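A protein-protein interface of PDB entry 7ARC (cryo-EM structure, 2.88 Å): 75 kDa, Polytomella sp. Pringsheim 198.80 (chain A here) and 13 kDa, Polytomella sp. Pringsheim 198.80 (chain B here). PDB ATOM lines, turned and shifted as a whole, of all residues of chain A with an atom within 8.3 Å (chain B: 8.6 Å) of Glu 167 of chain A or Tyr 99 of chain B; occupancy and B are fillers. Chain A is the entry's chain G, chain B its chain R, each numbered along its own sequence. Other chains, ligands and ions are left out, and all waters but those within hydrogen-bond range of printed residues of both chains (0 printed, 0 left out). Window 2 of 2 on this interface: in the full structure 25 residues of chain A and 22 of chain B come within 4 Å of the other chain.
CB of Leu 138 of chain A touches O of Val 97 of chain B, at 3.9 Å. Asp 139 of chain A touches Tyr 115 of chain B (CA to OH, 3.3 Å). O of Glu 167 of chain A touches OH of Tyr 99 of chain B, at 3.8 Å. Tyr 168 of chain A touches Tyr 99 of chain B. CB of Lys 169 of chain A touches CD1 of Tyr 99 of chain B (3.7 Å). Tyr 99 of chain B touches Ala 171 of chain A (O to CB, 3.9 Å). Ala 171 of chain A touches Ile 100 of chain B (CB to C, 3.9 Å). Ala 171 of chain A touches Ser 101 of chain B (CB to N, 3.5 Å). Ser 101 of chain B touches Val 172 of chain A (CB to C, 3.9 Å). Asn 186 of chain A touches Tyr 99 of chain B.
NZ of Lys 114 of chain B is in salt-bridge range of OD2 of Asp 139 of chain A (2.9 Å). OH of Tyr 115 of chain B sits close to O of Leu 138 of chain A (2.4 Å).
Of the 17 printed residues of chain A, 8 touch a printed residue of chain B. Printed residues of chain A that touch a printed residue of chain B: Leu 138, Asp 139, Glu 167, Tyr 168, Lys 169, Ala 171, Val 172 and Asn 186.
Of chain B, only Tyr 99 (3.8 Å) comes within 4 Å of Glu 167 of chain A. Of chain A, only Glu 167 (3.8 Å), Tyr 168 (3.3 Å), Lys 169 (3.7 Å), Ala 171 (3.9 Å) and Asn 186 (3.7 Å) come within 4 Å of Tyr 99 of chain B. Of the printed residues of chain A, Tyr 115 of chain B touches Leu 138 and Asp 139. Of the printed residues of chain A, Ile 100 of chain B touches Ala 171 (3.9 Å). Printed residues of chain B within 4 Å of Leu 138 of chain A: Val 97 (3.9 Å) and Tyr 115 (2.4 Å). Printed residues of chain A within 4 Å of Val 97 of chain B: Leu 138. Of the printed residues of chain B, Asn 186 of chain A touches Tyr 99. Leu 81 of chain B touches none of the printed residues of chain A. The nearest residue of chain B that does not touch Glu 167 of chain A is Val 97 of chain B (7.6 Å). The nearest residue of chain A that does not touch Tyr 99 of chain B is Arg 170 of chain A (4.7 Å). The nearest printed residue of chain A that does not touch Lys 114 of chain B is Asn 186 of chain A (6.0 Å).
O of Val 83 of chain B lies within hydrogen-bond range of N of Ile 100 of chain B (3.1 Å). The side-chain amino group (NZ) of Lys 169 of chain A sits at hydrogen-bond distance from the backbone carbonyl oxygen (O) of Ile 134 of chain A (2.8 Å). O of His 136 of chain A is in hydrogen-bond range of NZ of Lys 169 of chain A, 2.7 Å away. O of Arg 170 of chain A lies close to OD1 of Asn 186 of chain A, at 3.2 Å.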
ATOM      1  N   ILE A 134       7.822 -28.299  26.718  1.00  0.00           N
ATOM      2  CA  ILE A 134       8.458 -28.270  28.039  1.00  0.00           C
ATOM      3  C   ILE A 134       9.801 -28.993  28.024  1.00  0.00           C
ATOM      4  O   ILE A 134      10.769 -28.536  28.646  1.00  0.00           O
ATOM      5  CB  ILE A 134       7.530 -28.835  29.132  1.00  0.00           C
ATOM      6  CG1 ILE A 134       7.037 -30.237  28.783  1.00  0.00           C
ATOM      7  CG2 ILE A 134       6.388 -27.885  29.418  1.00  0.00           C
ATOM      8  CD1 ILE A 134       6.383 -30.933  29.947  1.00  0.00           C
ATOM      9  N   ASN A 135       9.895 -30.122  27.323  1.00  0.00           N
ATOM     10  CA  ASN A 135      11.128 -30.898  27.290  1.00  0.00           C
ATOM     11  C   ASN A 135      11.933 -30.700  26.015  1.00  0.00           C
ATOM     12  O   ASN A 135      12.936 -31.390  25.818  1.00  0.00           O
ATOM     13  CB  ASN A 135      10.828 -32.388  27.468  1.00  0.00           C
ATOM     14  CG  ASN A 135      10.462 -32.748  28.889  1.00  0.00           C
ATOM     15  OD1 ASN A 135      11.314 -32.760  29.774  1.00  0.00           O
ATOM     16  ND2 ASN A 135       9.194 -33.051  29.115  1.00  0.00           N
ATOM     17  N   HIS A 136      11.525 -29.784  25.148  1.00  0.00           N
ATOM     18  CA  HIS A 136      12.279 -29.549  23.929  1.00  0.00           C
ATOM     19  C   HIS A 136      13.552 -28.768  24.246  1.00  0.00           C
ATOM     20  O   HIS A 136      13.525 -27.843  25.062  1.00  0.00           O
ATOM     21  CB  HIS A 136      11.428 -28.792  22.915  1.00  0.00           C
ATOM     22  CG  HIS A 136      11.862 -28.988  21.498  1.00  0.00           C
ATOM     23  ND1 HIS A 136      11.708 -30.185  20.836  1.00  0.00           N
ATOM     24  CD2 HIS A 136      12.433 -28.140  20.613  1.00  0.00           C
ATOM     25  CE1 HIS A 136      12.174 -30.068  19.606  1.00  0.00           C
ATOM     26  NE2 HIS A 136      12.618 -28.836  19.446  1.00  0.00           N
ATOM     27  N   PRO A 137      14.678 -29.117  23.633  1.00  0.00           N
ATOM     28  CA  PRO A 137      15.912 -28.368  23.879  1.00  0.00           C
ATOM     29  C   PRO A 137      15.879 -26.996  23.226  1.00  0.00           C
ATOM     30  O   PRO A 137      15.275 -26.798  22.171  1.00  0.00           O
ATOM     31  CB  PRO A 137      16.987 -29.259  23.254  1.00  0.00           C
ATOM     32  CG  PRO A 137      16.277 -29.922  22.145  1.00  0.00           C
ATOM     33  CD  PRO A 137      14.895 -30.209  22.671  1.00  0.00           C
ATOM     34  N   LEU A 138      16.557 -26.042  23.863  1.00  0.00           N
ATOM     35  CA  LEU A 138      16.665 -24.683  23.334  1.00  0.00           C
ATOM     36  C   LEU A 138      17.773 -24.611  22.283  1.00  0.00           C
ATOM     37  O   LEU A 138      18.788 -23.936  22.439  1.00  0.00           O
ATOM     38  CB  LEU A 138      16.907 -23.681  24.456  1.00  0.00           C
ATOM     39  CG  LEU A 138      15.732 -23.247  25.333  1.00  0.00           C
ATOM     40  CD1 LEU A 138      15.290 -24.350  26.265  1.00  0.00           C
ATOM     41  CD2 LEU A 138      16.094 -22.004  26.115  1.00  0.00           C
ATOM     42  N   ASP A 139      17.555 -25.336  21.186  1.00  0.00           N
ATOM     43  CA  ASP A 139      18.562 -25.522  20.152  1.00  0.00           C
ATOM     44  C   ASP A 139      18.178 -24.856  18.839  1.00  0.00           C
ATOM     45  O   ASP A 139      18.720 -25.216  17.793  1.00  0.00           O
ATOM     46  CB  ASP A 139      18.813 -27.011  19.916  1.00  0.00           C
ATOM     47  CG  ASP A 139      19.595 -27.654  21.033  1.00  0.00           C
ATOM     48  OD1 ASP A 139      19.992 -26.939  21.974  1.00  0.00           O
ATOM     49  OD2 ASP A 139      19.813 -28.879  20.972  1.00  0.00           O
ATOM     50  N   ARG A 164       5.887 -21.623  31.665  1.00  0.00           N
ATOM     51  CA  ARG A 164       5.848 -21.765  33.112  1.00  0.00           C
ATOM     52  C   ARG A 164       6.686 -22.937  33.607  1.00  0.00           C
ATOM     53  O   ARG A 164       6.555 -23.333  34.770  1.00  0.00           O
ATOM     54  CB  ARG A 164       4.389 -21.906  33.555  1.00  0.00           C
ATOM     55  CG  ARG A 164       3.766 -23.191  33.057  1.00  0.00           C
ATOM     56  CD  ARG A 164       2.293 -23.336  33.394  1.00  0.00           C
ATOM     57  NE  ARG A 164       1.408 -22.403  32.711  1.00  0.00           N
ATOM     58  CZ  ARG A 164       0.116 -22.284  32.984  1.00  0.00           C
ATOM     59  NH1 ARG A 164      -0.482 -23.082  33.853  1.00  0.00           N
ATOM     60  NH2 ARG A 164      -0.599 -21.355  32.358  1.00  0.00           N
ATOM     61  N   PHE A 165       7.542 -23.498  32.757  1.00  0.00           N
ATOM     62  CA  PHE A 165       8.373 -24.641  33.114  1.00  0.00           C
ATOM     63  C   PHE A 165       9.718 -24.171  33.652  1.00  0.00           C
ATOM     64  O   PHE A 165      10.425 -23.407  32.988  1.00  0.00           O
ATOM     65  CB  PHE A 165       8.573 -25.541  31.895  1.00  0.00           C
ATOM     66  CG  PHE A 165       9.215 -26.858  32.207  1.00  0.00           C
ATOM     67  CD1 PHE A 165       8.552 -27.806  32.961  1.00  0.00           C
ATOM     68  CD2 PHE A 165      10.477 -27.156  31.727  1.00  0.00           C
ATOM     69  CE1 PHE A 165       9.139 -29.019  33.241  1.00  0.00           C
ATOM     70  CE2 PHE A 165      11.067 -28.367  32.004  1.00  0.00           C
ATOM     71  CZ  PHE A 165      10.398 -29.300  32.761  1.00  0.00           C
ATOM     72  N   ILE A 166      10.068 -24.624  34.854  1.00  0.00           N
ATOM     73  CA  ILE A 166      11.334 -24.280  35.487  1.00  0.00           C
ATOM     74  C   ILE A 166      12.157 -25.502  35.863  1.00  0.00           C
ATOM     75  O   ILE A 166      13.232 -25.351  36.451  1.00  0.00           O
ATOM     76  CB  ILE A 166      11.125 -23.381  36.722  1.00  0.00           C
ATOM     77  CG1 ILE A 166      10.306 -24.113  37.781  1.00  0.00           C
ATOM     78  CG2 ILE A 166      10.453 -22.077  36.326  1.00  0.00           C
ATOM     79  CD1 ILE A 166      10.254 -23.397  39.103  1.00  0.00           C
ATOM     80  N   GLU A 167      11.692 -26.705  35.543  1.00  0.00           N
ATOM     81  CA  GLU A 167      12.340 -27.931  35.977  1.00  0.00           C
ATOM     82  C   GLU A 167      13.396 -28.395  34.977  1.00  0.00           C
ATOM     83  O   GLU A 167      13.616 -27.789  33.926  1.00  0.00           O
ATOM     84  CB  GLU A 167      11.300 -29.023  36.208  1.00  0.00           C
ATOM     85  CG  GLU A 167      10.602 -28.915  37.543  1.00  0.00           C
ATOM     86  CD  GLU A 167       9.365 -28.053  37.475  1.00  0.00           C
ATOM     87  OE1 GLU A 167       8.959 -27.689  36.354  1.00  0.00           O
ATOM     88  OE2 GLU A 167       8.800 -27.736  38.540  1.00  0.00           O
ATOM     89  N   TYR A 168      14.069 -29.488  35.328  1.00  0.00           N
ATOM     90  CA  TYR A 168      15.098 -30.061  34.472  1.00  0.00           C
ATOM     91  C   TYR A 168      14.474 -30.729  33.254  1.00  0.00           C
ATOM     92  O   TYR A 168      13.490 -31.466  33.363  1.00  0.00           O
ATOM     93  CB  TYR A 168      15.912 -31.089  35.260  1.00  0.00           C
ATOM     94  CG  TYR A 168      17.143 -30.535  35.932  1.00  0.00           C
ATOM     95  CD1 TYR A 168      18.334 -30.395  35.239  1.00  0.00           C
ATOM     96  CD2 TYR A 168      17.111 -30.143  37.263  1.00  0.00           C
ATOM     97  CE1 TYR A 168      19.460 -29.886  35.848  1.00  0.00           C
ATOM     98  CE2 TYR A 168      18.233 -29.631  37.883  1.00  0.00           C
ATOM     99  CZ  TYR A 168      19.404 -29.505  37.170  1.00  0.00           C
ATOM    100  OH  TYR A 168      20.524 -28.995  37.783  1.00  0.00           O
ATOM    101  N   LYS A 169      15.059 -30.477  32.089  1.00  0.00           N
ATOM    102  CA  LYS A 169      14.603 -31.082  30.849  1.00  0.00           C
ATOM    103  C   LYS A 169      15.262 -32.439  30.640  1.00  0.00           C
ATOM    104  O   LYS A 169      16.289 -32.762  31.238  1.00  0.00           O
ATOM    105  CB  LYS A 169      14.884 -30.180  29.649  1.00  0.00           C
ATOM    106  CG  LYS A 169      14.149 -28.859  29.671  1.00  0.00           C
ATOM    107  CD  LYS A 169      14.433 -28.057  28.418  1.00  0.00           C
ATOM    108  CE  LYS A 169      13.644 -26.764  28.410  1.00  0.00           C
ATOM    109  NZ  LYS A 169      12.589 -26.761  27.362  1.00  0.00           N
ATOM    110  N   ARG A 170      14.647 -33.236  29.775  1.00  0.00           N
ATOM    111  CA  ARG A 170      15.153 -34.561  29.466  1.00  0.00           C
ATOM    112  C   ARG A 170      16.364 -34.470  28.548  1.00  0.00           C
ATOM    113  O   ARG A 170      16.501 -33.535  27.755  1.00  0.00           O
ATOM    114  CB  ARG A 170      14.049 -35.391  28.808  1.00  0.00           C
ATOM    115  CG  ARG A 170      14.406 -36.828  28.529  1.00  0.00           C
ATOM    116  CD  ARG A 170      13.267 -37.539  27.831  1.00  0.00           C
ATOM    117  NE  ARG A 170      12.990 -36.971  26.518  1.00  0.00           N
ATOM    118  CZ  ARG A 170      11.867 -36.343  26.197  1.00  0.00           C
ATOM    119  NH1 ARG A 170      10.900 -36.161  27.080  1.00  0.00           N
ATOM    120  NH2 ARG A 170      11.717 -35.872  24.963  1.00  0.00           N
ATOM    121  N   ALA A 171      17.251 -35.457  28.664  1.00  0.00           N
ATOM    122  CA  ALA A 171      18.497 -35.489  27.912  1.00  0.00           C
ATOM    123  C   ALA A 171      18.655 -36.857  27.272  1.00  0.00           C
ATOM    124  O   ALA A 171      18.463 -37.881  27.936  1.00  0.00           O
ATOM    125  CB  ALA A 171      19.693 -35.180  28.812  1.00  0.00           C
ATOM    126  N   VAL A 172      19.002 -36.875  25.990  1.00  0.00           N
ATOM    127  CA  VAL A 172      19.197 -38.111  25.244  1.00  0.00           C
ATOM    128  C   VAL A 172      20.589 -38.102  24.629  1.00  0.00           C
ATOM    129  O   VAL A 172      21.137 -37.045  24.301  1.00  0.00           O
ATOM    130  CB  VAL A 172      18.115 -38.295  24.155  1.00  0.00           C
ATOM    131  CG1 VAL A 172      18.140 -39.703  23.598  1.00  0.00           C
ATOM    132  CG2 VAL A 172      16.741 -37.979  24.712  1.00  0.00           C
ATOM    133  N   ALA A 173      21.164 -39.291  24.482  1.00  0.00           N
ATOM    134  CA  ALA A 173      22.461 -39.469  23.846  1.00  0.00           C
ATOM    135  C   ALA A 173      22.254 -39.986  22.428  1.00  0.00           C
ATOM    136  O   ALA A 173      21.596 -41.013  22.228  1.00  0.00           O
ATOM    137  CB  ALA A 173      23.335 -40.432  24.645  1.00  0.00           C
ATOM    138  N   ASN A 186      17.439 -35.506  21.257  1.00  0.00           N
ATOM    139  CA  ASN A 186      16.923 -34.651  22.314  1.00  0.00           C
ATOM    140  C   ASN A 186      15.785 -33.783  21.788  1.00  0.00           C
ATOM    141  O   ASN A 186      14.845 -33.475  22.528  1.00  0.00           O
ATOM    142  CB  ASN A 186      18.069 -33.813  22.883  1.00  0.00           C
ATOM    143  CG  ASN A 186      17.683 -33.051  24.129  1.00  0.00           C
ATOM    144  OD1 ASN A 186      16.544 -33.108  24.586  1.00  0.00           O
ATOM    145  ND2 ASN A 186      18.647 -32.340  24.701  1.00  0.00           N
ATOM    146  N   LEU B  81      23.507 -37.497  36.203  1.00  0.00           N
ATOM    147  CA  LEU B  81      23.399 -37.987  34.837  1.00  0.00           C
ATOM    148  C   LEU B  81      23.037 -36.887  33.851  1.00  0.00           C
ATOM    149  O   LEU B  81      22.957 -37.152  32.649  1.00  0.00           O
ATOM    150  CB  LEU B  81      22.376 -39.125  34.755  1.00  0.00           C
ATOM    151  CG  LEU B  81      22.797 -40.487  35.320  1.00  0.00           C
ATOM    152  CD1 LEU B  81      22.872 -40.492  36.842  1.00  0.00           C
ATOM    153  CD2 LEU B  81      21.851 -41.562  34.841  1.00  0.00           C
ATOM    154  N   VAL B  82      22.824 -35.664  34.331  1.00  0.00           N
ATOM    155  CA  VAL B  82      22.506 -34.514  33.494  1.00  0.00           C
ATOM    156  C   VAL B  82      23.203 -33.300  34.091  1.00  0.00           C
ATOM    157  O   VAL B  82      23.192 -33.106  35.311  1.00  0.00           O
ATOM    158  CB  VAL B  82      20.982 -34.283  33.394  1.00  0.00           C
ATOM    159  CG1 VAL B  82      20.678 -32.899  32.845  1.00  0.00           C
ATOM    160  CG2 VAL B  82      20.334 -35.348  32.526  1.00  0.00           C
ATOM    161  N   VAL B  83      23.811 -32.484  33.235  1.00  0.00           N
ATOM    162  CA  VAL B  83      24.432 -31.231  33.644  1.00  0.00           C
ATOM    163  C   VAL B  83      23.771 -30.084  32.890  1.00  0.00           C
ATOM    164  O   VAL B  83      23.490 -30.193  31.692  1.00  0.00           O
ATOM    165  CB  VAL B  83      25.961 -31.244  33.417  1.00  0.00           C
ATOM    166  CG1 VAL B  83      26.301 -31.330  31.937  1.00  0.00           C
ATOM    167  CG2 VAL B  83      26.605 -30.022  34.048  1.00  0.00           C
ATOM    168  N   ALA B  84      23.485 -29.002  33.607  1.00  0.00           N
ATOM    169  CA  ALA B  84      22.977 -27.779  33.001  1.00  0.00           C
ATOM    170  C   ALA B  84      24.155 -26.930  32.537  1.00  0.00           C
ATOM    171  O   ALA B  84      25.049 -26.614  33.329  1.00  0.00           O
ATOM    172  CB  ALA B  84      22.106 -27.006  33.989  1.00  0.00           C
ATOM    173  N   SER B  85      24.162 -26.570  31.255  1.00  0.00           N
ATOM    174  CA  SER B  85      25.242 -25.793  30.661  1.00  0.00           C
ATOM    175  C   SER B  85      24.695 -24.448  30.213  1.00  0.00           C
ATOM    176  O   SER B  85      23.829 -24.389  29.333  1.00  0.00           O
ATOM    177  CB  SER B  85      25.868 -26.536  29.478  1.00  0.00           C
ATOM    178  OG  SER B  85      27.088 -25.929  29.086  1.00  0.00           O
ATOM    179  N   HIS B  86      25.202 -23.371  30.813  1.00  0.00           N
ATOM    180  CA  HIS B  86      24.857 -22.015  30.405  1.00  0.00           C
ATOM    181  C   HIS B  86      25.979 -21.339  29.630  1.00  0.00           C
ATOM    182  O   HIS B  86      25.903 -20.132  29.377  1.00  0.00           O
ATOM    183  CB  HIS B  86      24.506 -21.171  31.631  1.00  0.00           C
ATOM    184  CG  HIS B  86      23.266 -21.617  32.336  1.00  0.00           C
ATOM    185  ND1 HIS B  86      23.283 -22.566  33.335  1.00  0.00           N
ATOM    186  CD2 HIS B  86      21.974 -21.241  32.194  1.00  0.00           C
ATOM    187  CE1 HIS B  86      22.052 -22.759  33.776  1.00  0.00           C
ATOM    188  NE2 HIS B  86      21.239 -21.966  33.101  1.00  0.00           N
ATOM    189  N   CYS B  95      25.453 -18.763  26.491  1.00  0.00           N
ATOM    190  CA  CYS B  95      24.612 -19.565  25.624  1.00  0.00           C
ATOM    191  C   CYS B  95      23.290 -19.906  26.306  1.00  0.00           C
ATOM    192  O   CYS B  95      23.181 -19.849  27.534  1.00  0.00           O
ATOM    193  CB  CYS B  95      25.342 -20.843  25.231  1.00  0.00           C
ATOM    194  SG  CYS B  95      25.333 -22.142  26.479  1.00  0.00           S
ATOM    195  N   PRO B  96      22.264 -20.256  25.527  1.00  0.00           N
ATOM    196  CA  PRO B  96      21.005 -20.705  26.131  1.00  0.00           C
ATOM    197  C   PRO B  96      21.216 -21.942  26.988  1.00  0.00           C
ATOM    198  O   PRO B  96      22.112 -22.748  26.738  1.00  0.00           O
ATOM    199  CB  PRO B  96      20.123 -21.011  24.916  1.00  0.00           C
ATOM    200  CG  PRO B  96      20.656 -20.112  23.853  1.00  0.00           C
ATOM    201  CD  PRO B  96      22.143 -20.111  24.067  1.00  0.00           C
ATOM    202  N   VAL B  97      20.382 -22.073  28.024  1.00  0.00           N
ATOM    203  CA  VAL B  97      20.501 -23.205  28.935  1.00  0.00           C
ATOM    204  C   VAL B  97      20.360 -24.502  28.152  1.00  0.00           C
ATOM    205  O   VAL B  97      19.484 -24.641  27.290  1.00  0.00           O
ATOM    206  CB  VAL B  97      19.473 -23.099  30.071  1.00  0.00           C
ATOM    207  CG1 VAL B  97      18.051 -23.195  29.539  1.00  0.00           C
ATOM    208  CG2 VAL B  97      19.733 -24.174  31.116  1.00  0.00           C
ATOM    209  N   GLU B  98      21.245 -25.451  28.432  1.00  0.00           N
ATOM    210  CA  GLU B  98      21.268 -26.727  27.738  1.00  0.00           C
ATOM    211  C   GLU B  98      21.432 -27.839  28.761  1.00  0.00           C
ATOM    212  O   GLU B  98      22.158 -27.685  29.747  1.00  0.00           O
ATOM    213  CB  GLU B  98      22.399 -26.768  26.703  1.00  0.00           C
ATOM    214  CG  GLU B  98      22.448 -28.033  25.873  1.00  0.00           C
ATOM    215  CD  GLU B  98      23.549 -27.997  24.835  1.00  0.00           C
ATOM    216  OE1 GLU B  98      24.283 -26.989  24.789  1.00  0.00           O
ATOM    217  OE2 GLU B  98      23.677 -28.969  24.063  1.00  0.00           O
ATOM    218  N   TYR B  99      20.746 -28.951  28.527  1.00  0.00           N
ATOM    219  CA  TYR B  99      20.795 -30.115  29.401  1.00  0.00           C
ATOM    220  C   TYR B  99      21.441 -31.261  28.636  1.00  0.00           C
ATOM    221  O   TYR B  99      20.900 -31.720  27.624  1.00  0.00           O
ATOM    222  CB  TYR B  99      19.393 -30.485  29.877  1.00  0.00           C
ATOM    223  CG  TYR B  99      18.728 -29.370  30.651  1.00  0.00           C
ATOM    224  CD1 TYR B  99      18.034 -28.365  29.994  1.00  0.00           C
ATOM    225  CD2 TYR B  99      18.816 -29.305  32.032  1.00  0.00           C
ATOM    226  CE1 TYR B  99      17.433 -27.339  30.689  1.00  0.00           C
ATOM    227  CE2 TYR B  99      18.218 -28.279  32.734  1.00  0.00           C
ATOM    228  CZ  TYR B  99      17.528 -27.301  32.059  1.00  0.00           C
ATOM    229  OH  TYR B  99      16.930 -26.279  32.757  1.00  0.00           O
ATOM    230  N   ILE B 100      22.591 -31.719  29.120  1.00  0.00           N
ATOM    231  CA  ILE B 100      23.434 -32.676  28.414  1.00  0.00           C
ATOM    232  C   ILE B 100      23.396 -34.006  29.149  1.00  0.00           C
ATOM    233  O   ILE B 100      23.530 -34.051  30.377  1.00  0.00           O
ATOM    234  CB  ILE B 100      24.878 -32.160  28.283  1.00  0.00           C
ATOM    235  CG1 ILE B 100      24.875 -30.676  27.915  1.00  0.00           C
ATOM    236  CG2 ILE B 100      25.644 -32.965  27.253  1.00  0.00           C
ATOM    237  CD1 ILE B 100      26.218 -30.011  28.046  1.00  0.00           C
ATOM    238  N   SER B 101      23.192 -35.083  28.396  1.00  0.00           N
ATOM    239  CA  SER B 101      23.182 -36.425  28.960  1.00  0.00           C
ATOM    240  C   SER B 101      24.597 -36.872  29.301  1.00  0.00           C
ATOM    241  O   SER B 101      25.501 -36.807  28.463  1.00  0.00           O
ATOM    242  CB  SER B 101      22.541 -37.404  27.980  1.00  0.00           C
ATOM    243  OG  SER B 101      22.551 -38.722  28.498  1.00  0.00           O
ATOM    244  N   LEU B 102      24.786 -37.330  30.535  1.00  0.00           N
ATOM    245  CA  LEU B 102      26.073 -37.821  31.007  1.00  0.00           C
ATOM    246  C   LEU B 102      26.178 -39.337  30.941  1.00  0.00           C
ATOM    247  O   LEU B 102      27.191 -39.894  31.372  1.00  0.00           O
ATOM    248  CB  LEU B 102      26.330 -37.357  32.445  1.00  0.00           C
ATOM    249  CG  LEU B 102      26.895 -35.953  32.681  1.00  0.00           C
ATOM    250  CD1 LEU B 102      28.278 -35.820  32.082  1.00  0.00           C
ATOM    251  CD2 LEU B 102      25.978 -34.870  32.165  1.00  0.00           C
ATOM    252  N   ALA B 111      30.956 -35.918  26.992  1.00  0.00           N
ATOM    253  CA  ALA B 111      29.866 -35.193  26.356  1.00  0.00           C
ATOM    254  C   ALA B 111      30.281 -33.749  26.106  1.00  0.00           C
ATOM    255  O   ALA B 111      31.147 -33.205  26.793  1.00  0.00           O
ATOM    256  CB  ALA B 111      28.610 -35.233  27.224  1.00  0.00           C
ATOM    257  N   VAL B 112      29.648 -33.123  25.117  1.00  0.00           N
ATOM    258  CA  VAL B 112      30.051 -31.804  24.643  1.00  0.00           C
ATOM    259  C   VAL B 112      28.848 -30.873  24.628  1.00  0.00           C
ATOM    260  O   VAL B 112      27.740 -31.278  24.257  1.00  0.00           O
ATOM    261  CB  VAL B 112      30.691 -31.886  23.240  1.00  0.00           C
ATOM    262  CG1 VAL B 112      31.128 -30.512  22.764  1.00  0.00           C
ATOM    263  CG2 VAL B 112      31.871 -32.832  23.259  1.00  0.00           C
ATOM    264  N   CYS B 113      29.069 -29.624  25.034  1.00  0.00           N
ATOM    265  CA  CYS B 113      28.078 -28.569  24.874  1.00  0.00           C
ATOM    266  C   CYS B 113      28.171 -28.007  23.461  1.00  0.00           C
ATOM    267  O   CYS B 113      29.233 -27.534  23.043  1.00  0.00           O
ATOM    268  CB  CYS B 113      28.299 -27.468  25.908  1.00  0.00           C
ATOM    269  SG  CYS B 113      27.133 -26.094  25.808  1.00  0.00           S
ATOM    270  N   LYS B 114      27.060 -28.066  22.728  1.00  0.00           N
ATOM    271  CA  LYS B 114      27.074 -27.682  21.320  1.00  0.00           C
ATOM    272  C   LYS B 114      27.324 -26.188  21.141  1.00  0.00           C
ATOM    273  O   LYS B 114      27.988 -25.778  20.182  1.00  0.00           O
ATOM    274  CB  LYS B 114      25.768 -28.120  20.662  1.00  0.00           C
ATOM    275  CG  LYS B 114      25.644 -29.635  20.594  1.00  0.00           C
ATOM    276  CD  LYS B 114      24.436 -30.097  19.808  1.00  0.00           C
ATOM    277  CE  LYS B 114      23.157 -29.881  20.593  1.00  0.00           C
ATOM    278  NZ  LYS B 114      21.979 -30.432  19.875  1.00  0.00           N
ATOM    279  N   TYR B 115      26.788 -25.360  22.036  1.00  0.00           N
ATOM    280  CA  TYR B 115      27.010 -23.920  21.937  1.00  0.00           C
ATOM    281  C   TYR B 115      28.453 -23.546  22.260  1.00  0.00           C
ATOM    282  O   TYR B 115      29.076 -22.759  21.540  1.00  0.00           O
ATOM    283  CB  TYR B 115      26.051 -23.176  22.861  1.00  0.00           C
ATOM    284  CG  TYR B 115      24.607 -23.177  22.416  1.00  0.00           C
ATOM    285  CD1 TYR B 115      24.153 -22.261  21.480  1.00  0.00           C
ATOM    286  CD2 TYR B 115      23.704 -24.094  22.925  1.00  0.00           C
ATOM    287  CE1 TYR B 115      22.838 -22.253  21.072  1.00  0.00           C
ATOM    288  CE2 TYR B 115      22.386 -24.094  22.518  1.00  0.00           C
ATOM    289  CZ  TYR B 115      21.961 -23.170  21.592  1.00  0.00           C
ATOM    290  OH  TYR B 115      20.651 -23.163  21.183  1.00  0.00           O
